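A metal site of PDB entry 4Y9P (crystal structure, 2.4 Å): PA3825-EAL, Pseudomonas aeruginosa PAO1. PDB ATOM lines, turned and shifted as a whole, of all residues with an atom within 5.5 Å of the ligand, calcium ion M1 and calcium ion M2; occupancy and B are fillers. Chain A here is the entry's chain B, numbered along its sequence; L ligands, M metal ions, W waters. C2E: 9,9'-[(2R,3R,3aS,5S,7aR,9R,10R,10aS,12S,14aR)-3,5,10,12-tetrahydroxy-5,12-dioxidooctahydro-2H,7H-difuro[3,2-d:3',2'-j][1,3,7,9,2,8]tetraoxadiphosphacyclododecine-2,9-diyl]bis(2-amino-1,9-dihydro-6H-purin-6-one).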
ATOM      1  N   GLN A  25      21.472 -10.947 -21.669  1.00  0.00           N
ATOM      2  CA  GLN A  25      21.100  -9.600 -22.061  1.00  0.00           C
ATOM      3  C   GLN A  25      19.745  -9.590 -22.835  1.00  0.00           C
ATOM      4  O   GLN A  25      19.611 -10.146 -23.965  1.00  0.00           O
ATOM      5  CB  GLN A  25      22.168  -8.919 -22.878  1.00  0.00           C
ATOM      6  CG  GLN A  25      21.749  -7.432 -23.067  1.00  0.00           C
ATOM      7  CD  GLN A  25      22.778  -6.541 -23.707  1.00  0.00           C
ATOM      8  OE1 GLN A  25      23.454  -6.966 -24.604  1.00  0.00           O
ATOM      9  NE2 GLN A  25      22.877  -5.289 -23.276  1.00  0.00           N
ATOM     10  N   GLU A  39      20.236 -12.544 -25.343  1.00  0.00           N
ATOM     11  CA  GLU A  39      21.553 -13.031 -25.785  1.00  0.00           C
ATOM     12  C   GLU A  39      22.259 -13.594 -24.524  1.00  0.00           C
ATOM     13  O   GLU A  39      22.358 -12.925 -23.523  1.00  0.00           O
ATOM     14  CB  GLU A  39      22.442 -11.922 -26.435  1.00  0.00           C
ATOM     15  CG  GLU A  39      23.700 -12.449 -27.118  1.00  0.00           C
ATOM     16  CD  GLU A  39      24.624 -11.389 -27.686  1.00  0.00           C
ATOM     17  OE1 GLU A  39      24.235 -10.194 -27.666  1.00  0.00           O
ATOM     18  OE2 GLU A  39      25.755 -11.759 -28.174  1.00  0.00           O
ATOM     19  N   VAL A  40      22.794 -14.776 -24.630  1.00  0.00           N
ATOM     20  CA  VAL A  40      23.532 -15.378 -23.562  1.00  0.00           C
ATOM     21  C   VAL A  40      24.949 -14.946 -23.748  1.00  0.00           C
ATOM     22  O   VAL A  40      25.540 -15.226 -24.797  1.00  0.00           O
ATOM     23  CB  VAL A  40      23.486 -16.907 -23.663  1.00  0.00           C
ATOM     24  CG1 VAL A  40      24.392 -17.486 -22.652  1.00  0.00           C
ATOM     25  CG2 VAL A  40      22.041 -17.375 -23.538  1.00  0.00           C
ATOM     26  N   LEU A  41      25.504 -14.270 -22.738  1.00  0.00           N
ATOM     27  CA  LEU A  41      26.901 -13.848 -22.723  1.00  0.00           C
ATOM     28  C   LEU A  41      27.739 -14.586 -21.668  1.00  0.00           C
ATOM     29  O   LEU A  41      27.367 -14.704 -20.510  1.00  0.00           O
ATOM     30  CB  LEU A  41      26.971 -12.380 -22.488  1.00  0.00           C
ATOM     31  CG  LEU A  41      26.462 -11.597 -23.686  1.00  0.00           C
ATOM     32  CD1 LEU A  41      26.140 -10.163 -23.299  1.00  0.00           C
ATOM     33  CD2 LEU A  41      27.396 -11.651 -24.865  1.00  0.00           C
ATOM     34  N   MET A  42      28.885 -15.082 -22.070  1.00  0.00           N
ATOM     35  CA  MET A  42      29.704 -15.817 -21.111  1.00  0.00           C
ATOM     36  C   MET A  42      30.357 -14.908 -20.069  1.00  0.00           C
ATOM     37  O   MET A  42      30.819 -13.806 -20.372  1.00  0.00           O
ATOM     38  CB  MET A  42      30.748 -16.620 -21.813  1.00  0.00           C
ATOM     39  CG  MET A  42      31.262 -17.740 -20.918  1.00  0.00           C
ATOM     40  SD  MET A  42      32.371 -18.870 -21.777  1.00  0.00           S
ATOM     41  CE  MET A  42      31.423 -19.460 -23.164  1.00  0.00           C
ATOM     42  N   ARG A  43      30.386 -15.358 -18.836  1.00  0.00           N
ATOM     43  CA  ARG A  43      31.147 -14.671 -17.800  1.00  0.00           C
ATOM     44  C   ARG A  43      31.969 -15.692 -17.059  1.00  0.00           C
ATOM     45  O   ARG A  43      31.567 -16.866 -16.934  1.00  0.00           O
ATOM     46  CB  ARG A  43      30.206 -13.988 -16.834  1.00  0.00           C
ATOM     47  CG  ARG A  43      29.455 -12.823 -17.436  1.00  0.00           C
ATOM     48  CD  ARG A  43      30.345 -11.633 -17.611  1.00  0.00           C
ATOM     49  NE  ARG A  43      29.673 -10.437 -18.148  1.00  0.00           N
ATOM     50  CZ  ARG A  43      29.488 -10.188 -19.452  1.00  0.00           C
ATOM     51  NH1 ARG A  43      29.839 -11.072 -20.395  1.00  0.00           N
ATOM     52  NH2 ARG A  43      28.872  -9.068 -19.815  1.00  0.00           N
ATOM     53  N   ARG A  53      35.660 -10.668 -17.856  1.00  0.00           N
ATOM     54  CA  ARG A  53      34.803 -10.447 -19.077  1.00  0.00           C
ATOM     55  C   ARG A  53      35.427 -11.163 -20.282  1.00  0.00           C
ATOM     56  O   ARG A  53      36.665 -11.382 -20.307  1.00  0.00           O
ATOM     57  CB  ARG A  53      34.605  -8.939 -19.406  1.00  0.00           C
ATOM     58  CG  ARG A  53      35.958  -8.217 -19.306  1.00  0.00           C
ATOM     59  CD  ARG A  53      36.096  -6.895 -20.034  1.00  0.00           C
ATOM     60  NE  ARG A  53      37.526  -6.613 -20.266  1.00  0.00           N
ATOM     61  CZ  ARG A  53      38.396  -6.210 -19.341  1.00  0.00           C
ATOM     62  NH1 ARG A  53      38.002  -6.020 -18.084  1.00  0.00           N
ATOM     63  NH2 ARG A  53      39.680  -5.996 -19.665  1.00  0.00           N
ATOM     64  N   PRO A  54      34.600 -11.528 -21.253  1.00  0.00           N
ATOM     65  CA  PRO A  54      34.938 -12.426 -22.389  1.00  0.00           C
ATOM     66  C   PRO A  54      36.158 -12.079 -23.220  1.00  0.00           C
ATOM     67  O   PRO A  54      36.903 -12.987 -23.616  1.00  0.00           O
ATOM     68  CB  PRO A  54      33.731 -12.354 -23.278  1.00  0.00           C
ATOM     69  CG  PRO A  54      32.601 -11.981 -22.381  1.00  0.00           C
ATOM     70  CD  PRO A  54      33.154 -11.210 -21.244  1.00  0.00           C
ATOM     71  N   ASP A  55      36.398 -10.797 -23.439  1.00  0.00           N
ATOM     72  CA  ASP A  55      37.534 -10.364 -24.283  1.00  0.00           C
ATOM     73  C   ASP A  55      38.887 -10.712 -23.675  1.00  0.00           C
ATOM     74  O   ASP A  55      39.833 -10.885 -24.395  1.00  0.00           O
ATOM     75  CB  ASP A  55      37.498  -8.897 -24.816  1.00  0.00           C
ATOM     76  CG  ASP A  55      36.275  -8.052 -24.348  1.00  0.00           C
ATOM     77  OD1 ASP A  55      35.346  -8.562 -23.664  1.00  0.00           O
ATOM     78  OD2 ASP A  55      36.254  -6.831 -24.660  1.00  0.00           O
ATOM     79  N   ILE A  58      37.941 -15.356 -24.174  1.00  0.00           N
ATOM     80  CA  ILE A  58      37.442 -16.014 -25.391  1.00  0.00           C
ATOM     81  C   ILE A  58      38.506 -16.212 -26.501  1.00  0.00           C
ATOM     82  O   ILE A  58      38.523 -17.262 -27.130  1.00  0.00           O
ATOM     83  CB  ILE A  58      36.183 -15.327 -25.948  1.00  0.00           C
ATOM     84  CG1 ILE A  58      34.989 -15.568 -24.996  1.00  0.00           C
ATOM     85  CG2 ILE A  58      35.819 -15.841 -27.345  1.00  0.00           C
ATOM     86  CD1 ILE A  58      34.437 -16.983 -24.941  1.00  0.00           C
ATOM     87  N   GLU A  62      39.202 -19.978 -28.143  1.00  0.00           N
ATOM     88  CA  GLU A  62      38.996 -20.238 -29.572  1.00  0.00           C
ATOM     89  C   GLU A  62      40.193 -20.849 -30.209  1.00  0.00           C
ATOM     90  O   GLU A  62      40.073 -21.849 -30.885  1.00  0.00           O
ATOM     91  CB  GLU A  62      38.559 -18.983 -30.319  1.00  0.00           C
ATOM     92  CG  GLU A  62      37.137 -18.581 -29.913  1.00  0.00           C
ATOM     93  CD  GLU A  62      36.568 -17.342 -30.609  1.00  0.00           C
ATOM     94  OE1 GLU A  62      37.328 -16.456 -31.029  1.00  0.00           O
ATOM     95  OE2 GLU A  62      35.333 -17.274 -30.724  1.00  0.00           O
ATOM     96  N   ILE A  67      36.812 -23.513 -26.364  1.00  0.00           N
ATOM     97  CA  ILE A  67      35.567 -22.810 -26.485  1.00  0.00           C
ATOM     98  C   ILE A  67      34.399 -23.768 -26.798  1.00  0.00           C
ATOM     99  O   ILE A  67      33.241 -23.482 -26.442  1.00  0.00           O
ATOM    100  CB  ILE A  67      35.681 -21.662 -27.544  1.00  0.00           C
ATOM    101  CG1 ILE A  67      34.441 -20.768 -27.545  1.00  0.00           C
ATOM    102  CG2 ILE A  67      35.887 -22.169 -28.976  1.00  0.00           C
ATOM    103  CD1 ILE A  67      34.176 -20.090 -26.224  1.00  0.00           C
ATOM    104  N   THR A  71      31.134 -23.922 -24.576  1.00  0.00           N
ATOM    105  CA  THR A  71      29.869 -23.491 -25.105  1.00  0.00           C
ATOM    106  C   THR A  71      28.773 -24.538 -24.839  1.00  0.00           C
ATOM    107  O   THR A  71      27.588 -24.194 -24.594  1.00  0.00           O
ATOM    108  CB  THR A  71      30.050 -23.257 -26.605  1.00  0.00           C
ATOM    109  OG1 THR A  71      31.034 -22.245 -26.786  1.00  0.00           O
ATOM    110  CG2 THR A  71      28.695 -22.823 -27.270  1.00  0.00           C
ATOM    111  N   LEU A  74      27.654 -24.141 -21.402  1.00  0.00           N
ATOM    112  CA  LEU A  74      26.852 -22.968 -21.269  1.00  0.00           C
ATOM    113  C   LEU A  74      25.448 -23.259 -21.745  1.00  0.00           C
ATOM    114  O   LEU A  74      24.467 -22.865 -21.093  1.00  0.00           O
ATOM    115  CB  LEU A  74      27.448 -21.808 -22.090  1.00  0.00           C
ATOM    116  CG  LEU A  74      27.041 -20.388 -21.671  1.00  0.00           C
ATOM    117  CD1 LEU A  74      27.786 -19.993 -20.394  1.00  0.00           C
ATOM    118  CD2 LEU A  74      27.362 -19.396 -22.791  1.00  0.00           C
ATOM    119  N   ASN A  98      26.589 -16.942 -28.838  1.00  0.00           N
ATOM    120  CA  ASN A  98      27.713 -16.576 -29.708  1.00  0.00           C
ATOM    121  C   ASN A  98      28.498 -17.847 -30.091  1.00  0.00           C
ATOM    122  O   ASN A  98      28.797 -18.612 -29.219  1.00  0.00           O
ATOM    123  CB  ASN A  98      28.595 -15.574 -28.982  1.00  0.00           C
ATOM    124  CG  ASN A  98      27.889 -14.247 -28.783  1.00  0.00           C
ATOM    125  OD1 ASN A  98      27.747 -13.465 -29.734  1.00  0.00           O
ATOM    126  ND2 ASN A  98      27.348 -14.035 -27.582  1.00  0.00           N
ATOM    127  N   ILE A  99      28.810 -18.060 -31.371  1.00  0.00           N
ATOM    128  CA  ILE A  99      29.581 -19.232 -31.758  1.00  0.00           C
ATOM    129  C   ILE A  99      30.846 -18.815 -32.562  1.00  0.00           C
ATOM    130  O   ILE A  99      30.866 -17.776 -33.236  1.00  0.00           O
ATOM    131  CB  ILE A  99      28.698 -20.413 -32.274  1.00  0.00           C
ATOM    132  CG1 ILE A  99      27.837 -20.107 -33.452  1.00  0.00           C
ATOM    133  CG2 ILE A  99      27.712 -20.884 -31.205  1.00  0.00           C
ATOM    134  CD1 ILE A  99      28.684 -19.766 -34.602  1.00  0.00           C
ATOM    135  N   SER A 100      31.935 -19.559 -32.366  1.00  0.00           N
ATOM    136  CA  SER A 100      33.200 -19.326 -33.053  1.00  0.00           C
ATOM    137  C   SER A 100      33.282 -20.009 -34.400  1.00  0.00           C
ATOM    138  O   SER A 100      32.482 -20.878 -34.697  1.00  0.00           O
ATOM    139  CB  SER A 100      34.350 -19.824 -32.183  1.00  0.00           C
ATOM    140  OG  SER A 100      33.981 -19.869 -30.821  1.00  0.00           O
ATOM    141  N   GLU A 130      24.890 -16.722 -33.283  1.00  0.00           N
ATOM    142  CA  GLU A 130      25.453 -15.479 -33.768  1.00  0.00           C
ATOM    143  C   GLU A 130      26.889 -15.712 -34.195  1.00  0.00           C
ATOM    144  O   GLU A 130      27.707 -16.244 -33.441  1.00  0.00           O
ATOM    145  CB  GLU A 130      25.387 -14.360 -32.730  1.00  0.00           C
ATOM    146  CG  GLU A 130      24.070 -14.238 -31.976  1.00  0.00           C
ATOM    147  CD  GLU A 130      23.990 -12.989 -31.097  1.00  0.00           C
ATOM    148  OE1 GLU A 130      25.054 -12.282 -30.906  1.00  0.00           O
ATOM    149  OE2 GLU A 130      22.842 -12.701 -30.646  1.00  0.00           O
ATOM    150  N   ASP A 160      26.540 -11.239 -36.375  1.00  0.00           N
ATOM    151  CA  ASP A 160      26.921 -10.372 -35.280  1.00  0.00           C
ATOM    152  C   ASP A 160      27.764  -9.228 -35.809  1.00  0.00           C
ATOM    153  O   ASP A 160      28.456  -9.374 -36.816  1.00  0.00           O
ATOM    154  CB  ASP A 160      27.771 -11.155 -34.289  1.00  0.00           C
ATOM    155  CG  ASP A 160      27.550 -10.723 -32.888  1.00  0.00           C
ATOM    156  OD1 ASP A 160      27.151  -9.540 -32.652  1.00  0.00           O
ATOM    157  OD2 ASP A 160      27.769 -11.588 -32.026  1.00  0.00           O
ATOM    158  N   ASP A 161      27.742  -8.113 -35.112  1.00  0.00           N
ATOM    159  CA  ASP A 161      28.653  -6.974 -35.427  1.00  0.00           C
ATOM    160  C   ASP A 161      28.706  -6.659 -36.949  1.00  0.00           C
ATOM    161  O   ASP A 161      29.760  -6.421 -37.500  1.00  0.00           O
ATOM    162  CB  ASP A 161      30.089  -7.242 -34.885  1.00  0.00           C
ATOM    163  CG  ASP A 161      30.104  -7.491 -33.356  1.00  0.00           C
ATOM    164  OD1 ASP A 161      29.233  -6.960 -32.554  1.00  0.00           O
ATOM    165  OD2 ASP A 161      30.989  -8.280 -32.979  1.00  0.00           O
ATOM    166  N   LYS A 181      22.690  -8.193 -36.936  1.00  0.00           N
ATOM    167  CA  LYS A 181      22.871  -7.384 -35.729  1.00  0.00           C
ATOM    168  C   LYS A 181      23.812  -6.214 -36.012  1.00  0.00           C
ATOM    169  O   LYS A 181      24.981  -6.383 -36.272  1.00  0.00           O
ATOM    170  CB  LYS A 181      23.393  -8.231 -34.570  1.00  0.00           C
ATOM    171  CG  LYS A 181      22.522  -9.457 -34.323  1.00  0.00           C
ATOM    172  CD  LYS A 181      22.887 -10.160 -33.026  1.00  0.00           C
ATOM    173  CE  LYS A 181      22.347  -9.446 -31.815  1.00  0.00           C
ATOM    174  NZ  LYS A 181      23.055  -9.918 -30.620  1.00  0.00           N
ATOM    175  N   ASP A 183      26.251  -3.568 -35.384  1.00  0.00           N
ATOM    176  CA  ASP A 183      27.249  -3.275 -34.368  1.00  0.00           C
ATOM    177  C   ASP A 183      26.977  -1.966 -33.576  1.00  0.00           C
ATOM    178  O   ASP A 183      26.543  -0.939 -34.120  1.00  0.00           O
ATOM    179  CB  ASP A 183      28.629  -3.156 -35.036  1.00  0.00           C
ATOM    180  CG  ASP A 183      29.752  -3.154 -34.027  1.00  0.00           C
ATOM    181  OD1 ASP A 183      29.924  -4.179 -33.293  1.00  0.00           O
ATOM    182  OD2 ASP A 183      30.394  -2.082 -33.897  1.00  0.00           O
ATOM    183  N   GLN A 184      27.288  -1.986 -32.295  1.00  0.00           N
ATOM    184  CA  GLN A 184      27.125  -0.770 -31.459  1.00  0.00           C
ATOM    185  C   GLN A 184      27.876   0.457 -31.943  1.00  0.00           C
ATOM    186  O   GLN A 184      27.527   1.550 -31.544  1.00  0.00           O
ATOM    187  CB  GLN A 184      27.431  -0.984 -29.981  1.00  0.00           C
ATOM    188  CG  GLN A 184      28.686  -1.707 -29.590  1.00  0.00           C
ATOM    189  CD  GLN A 184      28.539  -2.213 -28.173  1.00  0.00           C
ATOM    190  OE1 GLN A 184      29.233  -1.739 -27.257  1.00  0.00           O
ATOM    191  NE2 GLN A 184      27.612  -3.183 -27.966  1.00  0.00           N
ATOM    192  N   GLU A 217      22.246  -3.230 -31.583  1.00  0.00           N
ATOM    193  CA  GLU A 217      23.032  -3.436 -30.354  1.00  0.00           C
ATOM    194  C   GLU A 217      23.529  -2.122 -29.799  1.00  0.00           C
ATOM    195  O   GLU A 217      23.825  -1.227 -30.525  1.00  0.00           O
ATOM    196  CB  GLU A 217      24.255  -4.262 -30.682  1.00  0.00           C
ATOM    197  CG  GLU A 217      23.933  -5.682 -31.150  1.00  0.00           C
ATOM    198  CD  GLU A 217      25.133  -6.547 -31.336  1.00  0.00           C
ATOM    199  OE1 GLU A 217      26.291  -6.013 -31.391  1.00  0.00           O
ATOM    200  OE2 GLU A 217      24.898  -7.781 -31.427  1.00  0.00           O
ATOM    201  N   GLY A 218      23.691  -2.047 -28.501  1.00  0.00           N
ATOM    202  CA  GLY A 218      24.301  -0.916 -27.872  1.00  0.00           C
ATOM    203  C   GLY A 218      23.380   0.282 -27.745  1.00  0.00           C
ATOM    204  O   GLY A 218      23.850   1.394 -27.668  1.00  0.00           O
ATOM    205  N   VAL A 219      22.085   0.070 -27.666  1.00  0.00           N
ATOM    206  CA  VAL A 219      21.151   1.207 -27.457  1.00  0.00           C
ATOM    207  C   VAL A 219      21.260   1.642 -25.999  1.00  0.00           C
ATOM    208  O   VAL A 219      20.942   0.907 -25.123  1.00  0.00           O
ATOM    209  CB  VAL A 219      19.698   0.800 -27.752  1.00  0.00           C
ATOM    210  CG1 VAL A 219      18.730   1.944 -27.590  1.00  0.00           C
ATOM    211  CG2 VAL A 219      19.604   0.249 -29.168  1.00  0.00           C
ATOM    212  N   GLU A 220      21.771   2.828 -25.767  1.00  0.00           N
ATOM    213  CA  GLU A 220      21.906   3.397 -24.438  1.00  0.00           C
ATOM    214  C   GLU A 220      21.034   4.601 -24.171  1.00  0.00           C
ATOM    215  O   GLU A 220      20.761   4.928 -23.015  1.00  0.00           O
ATOM    216  CB  GLU A 220      23.361   3.817 -24.210  1.00  0.00           C
ATOM    217  CG  GLU A 220      24.325   2.657 -24.384  1.00  0.00           C
ATOM    218  CD  GLU A 220      25.777   3.079 -24.207  1.00  0.00           C
ATOM    219  OE1 GLU A 220      26.129   4.320 -24.167  1.00  0.00           O
ATOM    220  OE2 GLU A 220      26.593   2.148 -24.221  1.00  0.00           O
ATOM    221  N   GLN A 237      18.711  -3.879 -28.291  1.00  0.00           N
ATOM    222  CA  GLN A 237      19.533  -4.509 -27.284  1.00  0.00           C
ATOM    223  C   GLN A 237      20.527  -3.438 -26.785  1.00  0.00           C
ATOM    224  O   GLN A 237      21.033  -2.609 -27.586  1.00  0.00           O
ATOM    225  CB  GLN A 237      20.183  -5.712 -27.917  1.00  0.00           C
ATOM    226  CG  GLN A 237      21.122  -6.467 -27.026  1.00  0.00           C
ATOM    227  CD  GLN A 237      21.612  -7.773 -27.653  1.00  0.00           C
ATOM    228  OE1 GLN A 237      21.385  -8.060 -28.841  1.00  0.00           O
ATOM    229  NE2 GLN A 237      22.438  -8.478 -26.899  1.00  0.00           N
ATOM    230  N   GLY A 238      20.711  -3.355 -25.472  1.00  0.00           N
ATOM    231  CA  GLY A 238      21.652  -2.347 -24.923  1.00  0.00           C
ATOM    232  C   GLY A 238      21.304  -2.058 -23.479  1.00  0.00           C
ATOM    233  O   GLY A 238      20.260  -2.498 -23.022  1.00  0.00           O
ATOM    234  N   TYR A 239      22.174  -1.295 -22.793  1.00  0.00           N
ATOM    235  CA  TYR A 239      21.922  -0.851 -21.447  1.00  0.00           C
ATOM    236  C   TYR A 239      20.595  -0.132 -21.310  1.00  0.00           C
ATOM    237  O   TYR A 239      20.053  -0.195 -20.258  1.00  0.00           O
ATOM    238  CB  TYR A 239      23.049   0.068 -20.936  1.00  0.00           C
ATOM    239  CG  TYR A 239      24.407  -0.585 -20.953  1.00  0.00           C
ATOM    240  CD1 TYR A 239      24.532  -1.925 -20.959  1.00  0.00           C
ATOM    241  CD2 TYR A 239      25.584   0.169 -20.978  1.00  0.00           C
ATOM    242  CE1 TYR A 239      25.735  -2.528 -20.966  1.00  0.00           C
ATOM    243  CE2 TYR A 239      26.808  -0.434 -20.976  1.00  0.00           C
ATOM    244  CZ  TYR A 239      26.881  -1.810 -20.951  1.00  0.00           C
ATOM    245  OH  TYR A 239      28.074  -2.513 -20.928  1.00  0.00           O
ATOM    246  N   LEU A 240      20.041   0.473 -22.366  1.00  0.00           N
ATOM    247  CA  LEU A 240      18.717   1.131 -22.269  1.00  0.00           C
ATOM    248  C   LEU A 240      17.665   0.114 -21.991  1.00  0.00           C
ATOM    249  O   LEU A 240      16.802   0.365 -21.185  1.00  0.00           O
ATOM    250  CB  LEU A 240      18.329   1.925 -23.526  1.00  0.00           C
ATOM    251  CG  LEU A 240      17.089   2.852 -23.353  1.00  0.00           C
ATOM    252  CD1 LEU A 240      17.447   4.316 -23.184  1.00  0.00           C
ATOM    253  CD2 LEU A 240      16.148   2.824 -24.509  1.00  0.00           C
ATOM    254  N   GLY A 242      18.409  -3.265 -21.035  1.00  0.00           N
ATOM    255  CA  GLY A 242      18.937  -4.031 -19.932  1.00  0.00           C
ATOM    256  C   GLY A 242      20.383  -4.532 -20.155  1.00  0.00           C
ATOM    257  O   GLY A 242      20.692  -5.059 -21.204  1.00  0.00           O
ATOM    258  N   PRO A 244      23.565  -6.952 -19.564  1.00  0.00           N
ATOM    259  CA  PRO A 244      23.776  -8.353 -19.260  1.00  0.00           C
ATOM    260  C   PRO A 244      23.644  -8.600 -17.762  1.00  0.00           C
ATOM    261  O   PRO A 244      24.069  -7.793 -17.020  1.00  0.00           O
ATOM    262  CB  PRO A 244      25.223  -8.580 -19.665  1.00  0.00           C
ATOM    263  CG  PRO A 244      25.580  -7.517 -20.607  1.00  0.00           C
ATOM    264  CD  PRO A 244      24.732  -6.353 -20.232  1.00  0.00           C
HETATM  265  P1  C2E L   1      30.834  -8.871 -23.367  1.00  0.00           P
HETATM  266  O2P C2E L   1      29.830  -9.859 -22.795  1.00  0.00           O
HETATM  267  O1P C2E L   1      32.073  -8.445 -22.622  1.00  0.00           O
HETATM  268  O5' C2E L   1      31.281  -9.661 -24.678  1.00  0.00           O
HETATM  269  C5' C2E L   1      32.245  -9.153 -25.553  1.00  0.00           C
HETATM  270  C4' C2E L   1      32.351 -10.110 -26.745  1.00  0.00           C
HETATM  271  O4' C2E L   1      32.867 -11.359 -26.331  1.00  0.00           O
HETATM  272  C3' C2E L   1      31.047 -10.443 -27.452  1.00  0.00           C
HETATM  273  O3' C2E L   1      30.626  -9.401 -28.299  1.00  0.00           O
HETATM  274  C2' C2E L   1      31.446 -11.729 -28.153  1.00  0.00           C
HETATM  275  O2' C2E L   1      32.165 -11.446 -29.316  1.00  0.00           O
HETATM  276  C1' C2E L   1      32.356 -12.410 -27.146  1.00  0.00           C
HETATM  277  N9  C2E L   1      31.581 -13.398 -26.344  1.00  0.00           N
HETATM  278  C8  C2E L   1      30.858 -13.153 -25.219  1.00  0.00           C
HETATM  279  N7  C2E L   1      30.238 -14.277 -24.764  1.00  0.00           N
HETATM  280  C5  C2E L   1      30.567 -15.272 -25.626  1.00  0.00           C
HETATM  281  C6  C2E L   1      30.303 -16.730 -25.753  1.00  0.00           C
HETATM  282  O6  C2E L   1      29.587 -17.404 -24.956  1.00  0.00           O
HETATM  283  N1  C2E L   1      30.852 -17.342 -26.815  1.00  0.00           N
HETATM  284  C2  C2E L   1      31.645 -16.750 -27.701  1.00  0.00           C
HETATM  285  N2  C2E L   1      32.148 -17.491 -28.716  1.00  0.00           N
HETATM  286  N3  C2E L   1      31.936 -15.435 -27.634  1.00  0.00           N
HETATM  287  C4  C2E L   1      31.434 -14.677 -26.659  1.00  0.00           C
HETATM  288  P11 C2E L   1      29.166  -9.224 -28.849  1.00  0.00           P
HETATM  289  O21 C2E L   1      28.353 -10.498 -28.943  1.00  0.00           O
HETATM  290  O11 C2E L   1      29.427  -8.423 -30.086  1.00  0.00           O
HETATM  291  O5A C2E L   1      28.502  -8.092 -27.990  1.00  0.00           O
HETATM  292  C5A C2E L   1      27.858  -8.083 -26.777  1.00  0.00           C
HETATM  293  C4A C2E L   1      28.829  -7.233 -25.941  1.00  0.00           C
HETATM  294  O4A C2E L   1      28.499  -5.856 -25.825  1.00  0.00           O
HETATM  295  C3A C2E L   1      28.862  -7.719 -24.515  1.00  0.00           C
HETATM  296  O3A C2E L   1      30.162  -7.575 -24.014  1.00  0.00           O
HETATM  297  C2A C2E L   1      27.931  -6.812 -23.786  1.00  0.00           C
HETATM  298  O2A C2E L   1      28.200  -6.791 -22.393  1.00  0.00           O
HETATM  299  C1A C2E L   1      28.237  -5.491 -24.474  1.00  0.00           C
HETATM  300  N91 C2E L   1      27.067  -4.607 -24.454  1.00  0.00           N
HETATM  301  C81 C2E L   1      25.759  -4.934 -24.458  1.00  0.00           C
HETATM  302  N71 C2E L   1      24.931  -3.845 -24.457  1.00  0.00           N
HETATM  303  C51 C2E L   1      25.727  -2.786 -24.465  1.00  0.00           C
HETATM  304  C61 C2E L   1      25.539  -1.319 -24.498  1.00  0.00           C
HETATM  305  O61 C2E L   1      24.401  -0.816 -24.470  1.00  0.00           O
HETATM  306  N11 C2E L   1      26.647  -0.564 -24.499  1.00  0.00           N
HETATM  307  C21 C2E L   1      27.877  -1.122 -24.490  1.00  0.00           C
HETATM  308  N21 C2E L   1      28.951  -0.326 -24.515  1.00  0.00           N
HETATM  309  N31 C2E L   1      28.125  -2.471 -24.480  1.00  0.00           N
HETATM  310  C41 C2E L   1      27.112  -3.308 -24.458  1.00  0.00           C
HETATM  311 CA    CA M   1      27.472  -7.709 -31.282  1.00  0.00          CA
HETATM  312 CA    CA M   2      26.848 -11.360 -30.114  1.00  0.00          CA
HETATM  313 CA    CA M   3      31.794 -15.044 -32.464  1.00  0.00          CA
HETATM  314  O   HOH W   1      25.792  -9.334 -29.694  1.00  0.00           O
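OG of Ser 100 sits at hydrogen-bond distance from OE2 of Glu 62, 2.9 Å away.
The backbone carbonyl oxygen (O) of Glu 130 is in hydrogen-bond range of the backbone NH (N) of Ile 99 (3.0 Å).
NE2 of Gln 237 sits at hydrogen-bond distance from OE1 of Glu 39, at 2.6 Å.
The backbone NH (N) of Tyr 239 is in hydrogen-bond range of the backbone carbonyl oxygen (O) of Val 219 (3.4 Å).
The side-chain amide nitrogen (NE2) of Gln 25 is in hydrogen-bond range of the backbone carbonyl oxygen (O) of Gly 242, at 3.0 Å.
OE2 of Glu 130 lies within salt-bridge range of NZ of Lys 181 (2.8 Å).
N of Glu 39 lies within hydrogen-bond range of O of Gln 25 (2.8 Å).
OE1 of Gln 25 sits at hydrogen-bond distance from NE2 of Gln 237 (2.9 Å).
O1P of the ligand sits close to OD1 of Asp 55.
Leu 41 touches the ligand.
CD of Pro 54 touches O1P of the ligand, 3.3 Å away.
Ile 58 touches the ligand (CG2 to N3, 3.9 Å).
OE2 of Glu 62 touches N2 of the ligand, at 3.8 Å.
CD2 of Leu 74 touches O6 of the ligand (3.7 Å).
Ser 100 touches the ligand (OG to N2, 3.7 Å).
Gly 218 touches the ligand.
O of Val 219 touches O61 of the ligand, 3.9 Å away.
CA of Gly 238 touches O61 of the ligand, at 3.2 Å.
CG of Pro 244 touches O2A of the ligand, at 3.3 Å.
Hydrophobic or aromatic side chains within 4 Å of the ligand: Leu 41, Met 42, Pro 54, Ile 58, Leu 74, Tyr 239 and Pro 244.
Of the 33 residues printed, 21 come within 4 Å of the ligand.
Water W1 lies within hydrogen-bond range of the side-chain carboxylate (OE1) of Glu 39, the side-chain amino group (NZ) of Lys 181 and an oxygen (O5A) of the ligand.
Calcium ion M2 is bound by O21 of the ligand (2.1 Å), OD2 of Asp 160 (2.1 Å), OE1 of Glu 130 (2.2 Å), OE2 of Glu 39 (2.3 Å), OD1 of Asn 98 (2.3 Å) and water W1 (2.3 Å).
Slightly farther from calcium ion M2 lies OD1 of Asp 160 (3.1 Å).
Of the 33 residues printed, 3 come within 4 Å of calcium ion M1.
The nearest printed residue that does not touch calcium ion M1 is Asp 183 (4.7 Å).
Of the 33 residues printed, 4 come within 4 Å of calcium ion M2.
NE2 of Gln 25 is in hydrogen-bond range of N71 of the ligand.
The side-chain carboxylate (OE2) of Glu 220 sits at hydrogen-bond distance from a nitrogen (N11) of the ligand, 2.7 Å away.
A nitrogen (N7) of the ligand lies within hydrogen-bond range of the backbone NH (N) of Met 42 (3.1 Å).
N31 of the ligand lies close to OE1 of Gln 184 (3.1 Å).
N1 of the ligand lies within hydrogen-bond range of O of Asn 98 (3.4 Å).
The guanidinium group (NH1) of Arg 43 is in salt-bridge range of an oxygen (O2P) of the ligand (2.7 Å).
The backbone NH (N) of Tyr 239 is in hydrogen-bond range of an oxygen (O61) of the ligand, 2.8 Å away.
Calcium ion M1 is bound by OE1 of Glu 217 (2.1 Å), OD1 of Asp 161 (2.3 Å), OD1 of Asp 160 (2.3 Å), O11 of the ligand (2.4 Å), OE2 of Glu 217 (2.6 Å) and water W1 (2.8 Å).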
